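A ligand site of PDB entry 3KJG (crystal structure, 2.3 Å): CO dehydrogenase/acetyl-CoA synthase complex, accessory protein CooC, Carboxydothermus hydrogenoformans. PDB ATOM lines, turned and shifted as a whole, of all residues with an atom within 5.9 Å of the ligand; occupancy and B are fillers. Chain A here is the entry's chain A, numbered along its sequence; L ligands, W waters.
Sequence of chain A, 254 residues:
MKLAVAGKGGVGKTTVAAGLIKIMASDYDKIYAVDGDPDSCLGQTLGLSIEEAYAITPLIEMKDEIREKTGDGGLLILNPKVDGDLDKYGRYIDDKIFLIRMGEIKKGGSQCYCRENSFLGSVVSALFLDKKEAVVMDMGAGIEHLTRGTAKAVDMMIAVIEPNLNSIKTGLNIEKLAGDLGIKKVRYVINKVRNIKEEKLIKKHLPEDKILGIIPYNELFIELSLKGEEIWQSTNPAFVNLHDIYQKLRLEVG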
ATOM      1  N   GLY A   7       1.137 -21.996   7.563  1.00  0.00           N
ATOM      2  CA  GLY A   7       0.685 -21.724   8.917  1.00  0.00           C
ATOM      3  C   GLY A   7      -0.293 -20.569   8.954  1.00  0.00           C
ATOM      4  O   GLY A   7      -0.170 -19.623   8.172  1.00  0.00           O
ATOM      5  N   LYS A   8      -1.277 -20.645   9.837  1.00  0.00           N
ATOM      6  CA  LYS A   8      -2.248 -19.566   9.952  1.00  0.00           C
ATOM      7  C   LYS A   8      -1.482 -18.290  10.254  1.00  0.00           C
ATOM      8  O   LYS A   8      -0.393 -18.329  10.821  1.00  0.00           O
ATOM      9  CB  LYS A   8      -3.256 -19.861  11.071  1.00  0.00           C
ATOM     10  CG  LYS A   8      -4.303 -18.775  11.255  1.00  0.00           C
ATOM     11  CD  LYS A   8      -5.661 -19.362  11.623  1.00  0.00           C
ATOM     12  CE  LYS A   8      -6.715 -18.253  11.691  1.00  0.00           C
ATOM     13  NZ  LYS A   8      -8.116 -18.780  11.744  1.00  0.00           N
ATOM     14  N   GLY A   9      -2.038 -17.151   9.851  1.00  0.00           N
ATOM     15  CA  GLY A   9      -1.359 -15.890  10.090  1.00  0.00           C
ATOM     16  C   GLY A   9      -1.084 -15.602  11.551  1.00  0.00           C
ATOM     17  O   GLY A   9      -1.942 -15.799  12.405  1.00  0.00           O
ATOM     18  N   GLY A  10       0.123 -15.124  11.842  1.00  0.00           N
ATOM     19  CA  GLY A  10       0.467 -14.793  13.215  1.00  0.00           C
ATOM     20  C   GLY A  10       1.283 -15.868  13.908  1.00  0.00           C
ATOM     21  O   GLY A  10       1.888 -15.635  14.956  1.00  0.00           O
ATOM     22  N   VAL A  11       1.306 -17.060  13.330  1.00  0.00           N
ATOM     23  CA  VAL A  11       2.053 -18.152  13.929  1.00  0.00           C
ATOM     24  C   VAL A  11       3.572 -17.973  13.809  1.00  0.00           C
ATOM     25  O   VAL A  11       4.332 -18.621  14.527  1.00  0.00           O
ATOM     26  CB  VAL A  11       1.633 -19.513  13.295  1.00  0.00           C
ATOM     27  CG1 VAL A  11       2.492 -19.816  12.058  1.00  0.00           C
ATOM     28  CG2 VAL A  11       1.749 -20.621  14.332  1.00  0.00           C
ATOM     29  N   GLY A  12       4.014 -17.085  12.918  1.00  0.00           N
ATOM     30  CA  GLY A  12       5.434 -16.841  12.715  1.00  0.00           C
ATOM     31  C   GLY A  12       5.954 -17.602  11.512  1.00  0.00           C
ATOM     32  O   GLY A  12       7.158 -17.774  11.331  1.00  0.00           O
ATOM     33  N   LYS A  13       5.025 -18.057  10.693  1.00  0.00           N
ATOM     34  CA  LYS A  13       5.310 -18.825   9.488  1.00  0.00           C
ATOM     35  C   LYS A  13       6.347 -18.123   8.577  1.00  0.00           C
ATOM     36  O   LYS A  13       7.300 -18.745   8.095  1.00  0.00           O
ATOM     37  CB  LYS A  13       3.974 -19.070   8.765  1.00  0.00           C
ATOM     38  CG  LYS A  13       4.038 -19.671   7.391  1.00  0.00           C
ATOM     39  CD  LYS A  13       4.154 -18.592   6.334  1.00  0.00           C
ATOM     40  CE  LYS A  13       2.995 -17.637   6.416  1.00  0.00           C
ATOM     41  NZ  LYS A  13       3.408 -16.301   5.929  1.00  0.00           N
ATOM     42  N   THR A  14       6.172 -16.818   8.358  1.00  0.00           N
ATOM     43  CA  THR A  14       7.078 -16.059   7.513  1.00  0.00           C
ATOM     44  C   THR A  14       8.465 -15.985   8.137  1.00  0.00           C
ATOM     45  O   THR A  14       9.473 -16.036   7.436  1.00  0.00           O
ATOM     46  CB  THR A  14       6.579 -14.616   7.287  1.00  0.00           C
ATOM     47  OG1 THR A  14       5.303 -14.650   6.622  1.00  0.00           O
ATOM     48  CG2 THR A  14       7.570 -13.836   6.426  1.00  0.00           C
ATOM     49  N   THR A  15       8.502 -15.844   9.463  1.00  0.00           N
ATOM     50  CA  THR A  15       9.766 -15.746  10.176  1.00  0.00           C
ATOM     51  C   THR A  15      10.534 -17.058  10.061  1.00  0.00           C
ATOM     52  O   THR A  15      11.745 -17.049   9.873  1.00  0.00           O
ATOM     53  CB  THR A  15       9.548 -15.409  11.670  1.00  0.00           C
ATOM     54  OG1 THR A  15       9.031 -14.079  11.795  1.00  0.00           O
ATOM     55  CG2 THR A  15      10.874 -15.497  12.435  1.00  0.00           C
ATOM     56  N   VAL A  16       9.833 -18.168  10.164  1.00  0.00           N
ATOM     57  CA  VAL A  16      10.479 -19.459  10.038  1.00  0.00           C
ATOM     58  C   VAL A  16      10.998 -19.655   8.613  1.00  0.00           C
ATOM     59  O   VAL A  16      12.147 -20.062   8.419  1.00  0.00           O
ATOM     60  CB  VAL A  16       9.497 -20.594  10.403  1.00  0.00           C
ATOM     61  CG1 VAL A  16      10.108 -21.960  10.083  1.00  0.00           C
ATOM     62  CG2 VAL A  16       9.157 -20.521  11.876  1.00  0.00           C
ATOM     63  N   ASP A  37       2.380 -15.354   0.465  1.00  0.00           N
ATOM     64  CA  ASP A  37       1.446 -14.850   1.483  1.00  0.00           C
ATOM     65  C   ASP A  37       1.502 -13.327   1.553  1.00  0.00           C
ATOM     66  O   ASP A  37       2.435 -12.755   2.123  1.00  0.00           O
ATOM     67  CB  ASP A  37       1.771 -15.430   2.858  1.00  0.00           C
ATOM     68  CG  ASP A  37       0.947 -14.783   3.964  1.00  0.00           C
ATOM     69  OD1 ASP A  37       1.225 -15.063   5.144  1.00  0.00           O
ATOM     70  OD2 ASP A  37       0.023 -13.990   3.648  1.00  0.00           O
ATOM     71  N   ASP A  39      -0.305 -11.138   3.303  1.00  0.00           N
ATOM     72  CA  ASP A  39      -0.425 -10.563   4.643  1.00  0.00           C
ATOM     73  C   ASP A  39       0.885 -10.283   5.373  1.00  0.00           C
ATOM     74  O   ASP A  39       0.929  -9.451   6.279  1.00  0.00           O
ATOM     75  CB  ASP A  39      -1.313 -11.448   5.504  1.00  0.00           C
ATOM     76  CG  ASP A  39      -2.654 -11.696   4.849  1.00  0.00           C
ATOM     77  OD1 ASP A  39      -3.212 -10.742   4.269  1.00  0.00           O
ATOM     78  OD2 ASP A  39      -3.147 -12.850   4.920  1.00  0.00           O
ATOM     79  N   SER A  40       1.953 -10.977   4.980  1.00  0.00           N
ATOM     80  CA  SER A  40       3.265 -10.761   5.580  1.00  0.00           C
ATOM     81  C   SER A  40       4.319 -10.631   4.494  1.00  0.00           C
ATOM     82  O   SER A  40       4.185 -11.209   3.408  1.00  0.00           O
ATOM     83  CB  SER A  40       3.612 -11.890   6.537  1.00  0.00           C
ATOM     84  OG  SER A  40       2.934 -11.715   7.774  1.00  0.00           O
ATOM     85  N   CYS A  41       5.372  -9.866   4.767  1.00  0.00           N
ATOM     86  CA  CYS A  41       6.415  -9.639   3.788  1.00  0.00           C
ATOM     87  C   CYS A  41       7.681 -10.468   3.999  1.00  0.00           C
ATOM     88  O   CYS A  41       8.501 -10.151   4.847  1.00  0.00           O
ATOM     89  CB  CYS A  41       6.771  -8.150   3.758  1.00  0.00           C
ATOM     90  SG  CYS A  41       7.849  -7.666   2.398  1.00  0.00           S
ATOM     91  N   THR A  45      11.172  -9.405   6.135  1.00  0.00           N
ATOM     92  CA  THR A  45      11.623 -10.376   7.124  1.00  0.00           C
ATOM     93  C   THR A  45      12.993 -10.918   6.755  1.00  0.00           C
ATOM     94  O   THR A  45      13.764 -11.358   7.603  1.00  0.00           O
ATOM     95  CB  THR A  45      10.649 -11.546   7.234  1.00  0.00           C
ATOM     96  OG1 THR A  45       9.338 -11.024   7.510  1.00  0.00           O
ATOM     97  CG2 THR A  45      11.046 -12.484   8.342  1.00  0.00           C
ATOM     98  N   ASP A 138       6.494 -19.821   1.199  1.00  0.00           N
ATOM     99  CA  ASP A 138       5.668 -19.765   2.390  1.00  0.00           C
ATOM    100  C   ASP A 138       4.236 -19.513   1.916  1.00  0.00           C
ATOM    101  O   ASP A 138       4.034 -18.967   0.846  1.00  0.00           O
ATOM    102  CB  ASP A 138       6.117 -18.663   3.355  1.00  0.00           C
ATOM    103  CG  ASP A 138       5.669 -17.275   2.920  1.00  0.00           C
ATOM    104  OD1 ASP A 138       5.505 -16.391   3.796  1.00  0.00           O
ATOM    105  OD2 ASP A 138       5.505 -17.043   1.698  1.00  0.00           O
ATOM    106  N   ASN A 191       6.318 -22.818  17.084  1.00  0.00           N
ATOM    107  CA  ASN A 191       6.969 -21.556  17.326  1.00  0.00           C
ATOM    108  C   ASN A 191       6.342 -20.849  18.500  1.00  0.00           C
ATOM    109  O   ASN A 191       5.222 -21.180  18.899  1.00  0.00           O
ATOM    110  CB  ASN A 191       6.871 -20.691  16.067  1.00  0.00           C
ATOM    111  CG  ASN A 191       7.684 -19.413  16.172  1.00  0.00           C
ATOM    112  OD1 ASN A 191       8.726 -19.377  16.843  1.00  0.00           O
ATOM    113  ND2 ASN A 191       7.244 -18.361  15.468  1.00  0.00           N
ATOM    114  N   LYS A 192       7.079 -19.904  19.083  1.00  0.00           N
ATOM    115  CA  LYS A 192       6.584 -19.122  20.208  1.00  0.00           C
ATOM    116  C   LYS A 192       6.194 -19.957  21.437  1.00  0.00           C
ATOM    117  O   LYS A 192       5.169 -19.693  22.040  1.00  0.00           O
ATOM    118  CB  LYS A 192       5.362 -18.311  19.781  1.00  0.00           C
ATOM    119  CG  LYS A 192       5.610 -17.297  18.666  1.00  0.00           C
ATOM    120  CD  LYS A 192       4.307 -16.601  18.260  1.00  0.00           C
ATOM    121  CE  LYS A 192       4.591 -15.341  17.460  1.00  0.00           C
ATOM    122  NZ  LYS A 192       3.345 -14.646  16.994  1.00  0.00           N
ATOM    123  N   ILE A 215      10.692 -23.411  18.558  1.00  0.00           N
ATOM    124  CA  ILE A 215      11.301 -22.096  18.617  1.00  0.00           C
ATOM    125  C   ILE A 215      10.659 -21.313  19.755  1.00  0.00           C
ATOM    126  O   ILE A 215       9.449 -21.047  19.736  1.00  0.00           O
ATOM    127  CB  ILE A 215      11.135 -21.325  17.303  1.00  0.00           C
ATOM    128  CG1 ILE A 215      11.792 -22.109  16.163  1.00  0.00           C
ATOM    129  CG2 ILE A 215      11.789 -19.962  17.418  1.00  0.00           C
ATOM    130  CD1 ILE A 215      11.698 -21.414  14.824  1.00  0.00           C
ATOM    131  N   PRO A 216      11.465 -20.935  20.760  1.00  0.00           N
ATOM    132  CA  PRO A 216      10.982 -20.177  21.917  1.00  0.00           C
ATOM    133  C   PRO A 216      10.460 -18.814  21.532  1.00  0.00           C
ATOM    134  O   PRO A 216      10.810 -18.278  20.491  1.00  0.00           O
ATOM    135  CB  PRO A 216      12.238 -20.047  22.785  1.00  0.00           C
ATOM    136  CG  PRO A 216      13.096 -21.217  22.370  1.00  0.00           C
ATOM    137  CD  PRO A 216      12.900 -21.229  20.874  1.00  0.00           C
ATOM    138  N   TYR A 217       9.592 -18.279  22.381  1.00  0.00           N
ATOM    139  CA  TYR A 217       9.068 -16.947  22.162  1.00  0.00           C
ATOM    140  C   TYR A 217      10.253 -16.064  22.537  1.00  0.00           C
ATOM    141  O   TYR A 217      10.984 -16.385  23.474  1.00  0.00           O
ATOM    142  CB  TYR A 217       7.917 -16.667  23.122  1.00  0.00           C
ATOM    143  CG  TYR A 217       7.398 -15.259  23.030  1.00  0.00           C
ATOM    144  CD1 TYR A 217       6.440 -14.918  22.090  1.00  0.00           C
ATOM    145  CD2 TYR A 217       7.929 -14.256  23.825  1.00  0.00           C
ATOM    146  CE1 TYR A 217       6.009 -13.607  21.940  1.00  0.00           C
ATOM    147  CE2 TYR A 217       7.523 -12.944  23.701  1.00  0.00           C
ATOM    148  CZ  TYR A 217       6.555 -12.625  22.755  1.00  0.00           C
ATOM    149  OH  TYR A 217       6.142 -11.318  22.627  1.00  0.00           O
ATOM    150  N   ASN A 218      10.482 -14.981  21.808  1.00  0.00           N
ATOM    151  CA  ASN A 218      11.602 -14.102  22.116  1.00  0.00           C
ATOM    152  C   ASN A 218      11.312 -12.684  21.682  1.00  0.00           C
ATOM    153  O   ASN A 218      10.901 -12.447  20.541  1.00  0.00           O
ATOM    154  CB  ASN A 218      12.876 -14.591  21.417  1.00  0.00           C
ATOM    155  CG  ASN A 218      14.140 -13.965  21.997  1.00  0.00           C
ATOM    156  OD1 ASN A 218      14.206 -12.753  22.197  1.00  0.00           O
ATOM    157  ND2 ASN A 218      15.129 -14.792  22.275  1.00  0.00           N
ATOM    158  N   GLU A 219      11.526 -11.734  22.590  1.00  0.00           N
ATOM    159  CA  GLU A 219      11.275 -10.333  22.303  1.00  0.00           C
ATOM    160  C   GLU A 219      12.089  -9.845  21.108  1.00  0.00           C
ATOM    161  O   GLU A 219      11.633  -8.995  20.351  1.00  0.00           O
ATOM    162  CB  GLU A 219      11.575  -9.483  23.539  1.00  0.00           C
ATOM    163  CG  GLU A 219      10.383  -8.697  24.044  1.00  0.00           C
ATOM    164  CD  GLU A 219       9.186  -9.574  24.370  1.00  0.00           C
ATOM    165  OE1 GLU A 219       8.124  -9.024  24.750  1.00  0.00           O
ATOM    166  OE2 GLU A 219       9.300 -10.808  24.245  1.00  0.00           O
ATOM    167  N   PHE A 221      12.678 -11.016  18.214  1.00  0.00           N
ATOM    168  CA  PHE A 221      11.940 -11.087  16.956  1.00  0.00           C
ATOM    169  C   PHE A 221      11.067  -9.859  16.721  1.00  0.00           C
ATOM    170  O   PHE A 221      10.821  -9.482  15.589  1.00  0.00           O
ATOM    171  CB  PHE A 221      11.078 -12.353  16.909  1.00  0.00           C
ATOM    172  CG  PHE A 221      11.863 -13.594  16.624  1.00  0.00           C
ATOM    173  CD1 PHE A 221      12.486 -13.774  15.401  1.00  0.00           C
ATOM    174  CD2 PHE A 221      12.014 -14.569  17.607  1.00  0.00           C
ATOM    175  CE1 PHE A 221      13.244 -14.906  15.140  1.00  0.00           C
ATOM    176  CE2 PHE A 221      12.767 -15.710  17.366  1.00  0.00           C
ATOM    177  CZ  PHE A 221      13.389 -15.875  16.128  1.00  0.00           C
ATOM    178  N   ILE A 222      10.610  -9.249  17.803  1.00  0.00           N
ATOM    179  CA  ILE A 222       9.784  -8.033  17.718  1.00  0.00           C
ATOM    180  C   ILE A 222      10.656  -6.785  17.512  1.00  0.00           C
ATOM    181  O   ILE A 222      10.354  -5.933  16.675  1.00  0.00           O
ATOM    182  CB  ILE A 222       8.909  -7.911  19.005  1.00  0.00           C
ATOM    183  CG1 ILE A 222       7.579  -8.650  18.793  1.00  0.00           C
ATOM    184  CG2 ILE A 222       8.654  -6.460  19.349  1.00  0.00           C
ATOM    185  CD1 ILE A 222       6.950  -9.207  20.060  1.00  0.00           C
ATOM    186  N   SER A 225      12.629  -6.957  14.255  1.00  0.00           N
ATOM    187  CA  SER A 225      11.652  -6.811  13.183  1.00  0.00           C
ATOM    188  C   SER A 225      11.593  -5.375  12.650  1.00  0.00           C
ATOM    189  O   SER A 225      11.752  -5.166  11.449  1.00  0.00           O
ATOM    190  CB  SER A 225      10.264  -7.264  13.654  1.00  0.00           C
ATOM    191  OG  SER A 225       9.592  -6.235  14.350  1.00  0.00           O
HETATM  192  P1  LIG L   1       2.984 -14.947   9.792  1.00  0.00           P
HETATM  193  O1  LIG L   1       4.090 -15.144   8.845  1.00  0.00           O
HETATM  194  O2  LIG L   1       1.876 -13.802   9.593  1.00  0.00           O
HETATM  195  O3  LIG L   1       2.590 -16.041  10.912  1.00  0.00           O
HETATM  196  P2  LIG L   1       5.254 -13.553  10.610  1.00  0.00           P
HETATM  197  O4  LIG L   1       5.374 -12.228   9.956  1.00  0.00           O
HETATM  198  O5  LIG L   1       6.334 -14.554  10.713  1.00  0.00           O
HETATM  199  O6  LIG L   1       3.761 -14.085  10.902  1.00  0.00           O
HETATM  200  O7  LIG L   1       5.431 -13.046  12.124  1.00  0.00           O
HETATM  201  C1  LIG L   1       4.352 -12.446  12.858  1.00  0.00           C
HETATM  202  C2  LIG L   1       4.946 -11.836  14.131  1.00  0.00           C
HETATM  203  O8  LIG L   1       5.426 -12.888  14.984  1.00  0.00           O
HETATM  204  C3  LIG L   1       6.164 -11.023  13.714  1.00  0.00           C
HETATM  205  O9  LIG L   1       6.073  -9.674  14.211  1.00  0.00           O
HETATM  206  C4  LIG L   1       7.336 -11.772  14.344  1.00  0.00           C
HETATM  207  O10 LIG L   1       8.290 -10.809  14.829  1.00  0.00           O
HETATM  208  C5  LIG L   1       6.685 -12.463  15.539  1.00  0.00           C
HETATM  209  N1  LIG L   1       7.446 -13.680  15.905  1.00  0.00           N
HETATM  210  C6  LIG L   1       7.644 -14.687  15.060  1.00  0.00           C
HETATM  211  N2  LIG L   1       8.275 -15.679  15.667  1.00  0.00           N
HETATM  212  C7  LIG L   1       8.492 -15.318  16.926  1.00  0.00           C
HETATM  213  C8  LIG L   1       9.084 -15.942  18.001  1.00  0.00           C
HETATM  214  N3  LIG L   1       9.549 -17.184  17.895  1.00  0.00           N
HETATM  215  N4  LIG L   1       9.153 -15.291  19.176  1.00  0.00           N
HETATM  216  C9  LIG L   1       8.660 -14.079  19.297  1.00  0.00           C
HETATM  217  N5  LIG L   1       8.075 -13.452  18.280  1.00  0.00           N
HETATM  218  C10 LIG L   1       7.971 -14.028  17.083  1.00  0.00           C
HETATM  219  O   HOH W   1       0.170 -14.474   7.491  1.00  0.00           O
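The backbone NH of Asn 218 lies within hydrogen-bond range of a nitrogen (N4) of the ligand.
The backbone NH (N) of Gly 12 sits at hydrogen-bond distance from an oxygen (O3) of the ligand (2.7 Å).
O3 of the ligand is in hydrogen-bond range of N of Lys 13.
An oxygen (O5) of the ligand is in hydrogen-bond range of the side-chain hydroxyl (OG1) of Thr 15, 2.9 Å away.
The backbone NH (N) of Thr 15 is in hydrogen-bond range of an oxygen (O5) of the ligand, at 2.8 Å.
O8 of the ligand is in hydrogen-bond range of NZ of Lys 192, 3.4 Å away.
An oxygen (O10) of the ligand lies within hydrogen-bond range of the backbone carbonyl oxygen (O) of Phe 221, 3.0 Å away.
An oxygen (O1) of the ligand lies within hydrogen-bond range of the side-chain hydroxyl (OG1) of Thr 14 (2.6 Å).
The backbone NH (N) of Thr 14 sits at hydrogen-bond distance from an oxygen (O1) of the ligand (2.7 Å).
The side-chain amide oxygen of Asn 191 sits at hydrogen-bond distance from a nitrogen (N3) of the ligand (2.6 Å).
The side-chain hydroxyl (OG) of Ser 40 is in hydrogen-bond range of an oxygen (O2) of the ligand (3.0 Å).
The backbone NH of Gly 10 lies within hydrogen-bond range of an oxygen (O3) of the ligand (2.8 Å).
N of Val 11 is in hydrogen-bond range of O3 of the ligand (2.9 Å).
An oxygen (O1) of the ligand lies within salt-bridge range of the side-chain amino group (NZ) of Lys 13 (3.2 Å).
O of Pro 216 is in hydrogen-bond range of N3 of the ligand (3.1 Å).
The side-chain carboxylate (OD1) of Asp 138 is in salt-bridge range of the side-chain amino group (NZ) of Lys 13 (3.0 Å).
The side-chain amino group (NZ) of Lys 13 sits at hydrogen-bond distance from the side-chain hydroxyl (OG1) of Thr 14, 2.6 Å away.
The side-chain amide nitrogen (ND2) of Asn 191 lies within hydrogen-bond range of the backbone carbonyl oxygen (O) of Val 11 (3.1 Å).
The backbone carbonyl oxygen of Ile 215 sits at hydrogen-bond distance from the backbone NH of Lys 192 (2.7 Å).
OD1 of Asp 37 lies within salt-bridge range of NZ of Lys 13.
The backbone carbonyl oxygen (O) of Gly 10 is in hydrogen-bond range of the side-chain amino group (NZ) of Lys 192 (2.7 Å).
The side-chain amide oxygen of Asn 191 lies close to the backbone carbonyl oxygen of Ile 215, 3.4 Å away.
The side-chain hydroxyl (OG1) of Thr 14 lies within hydrogen-bond range of the side-chain carboxylate (OD1) of Asp 138 (3.3 Å).
Lys 8 touches the ligand (O to O3, 3.8 Å).
Gly 9 touches the ligand.
Ile 215 touches the ligand.
Tyr 217 touches the ligand.
Hydrophobic or aromatic side chains that line the ligand: Val 11, Ile 215, Tyr 217 and Phe 221.
16 residues have an atom within 4 Å of the ligand: Lys 8, Gly 9, Gly 10, Val 11, Gly 12, Lys 13, Thr 14, Thr 15, Ser 40, Asn 191, Lys 192, Ile 215, Pro 216, Tyr 217, Asn 218 and Phe 221.
Along chain A the residues within 4 Å of the ligand span positions 8 to 221.
The nearest printed residue that does not touch the ligand is Ile 222 (4.1 Å).
Water W1 bridges the side-chain carboxylate of Asp 37 (2.6 Å) and an oxygen (O2) of the ligand (2.8 Å).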
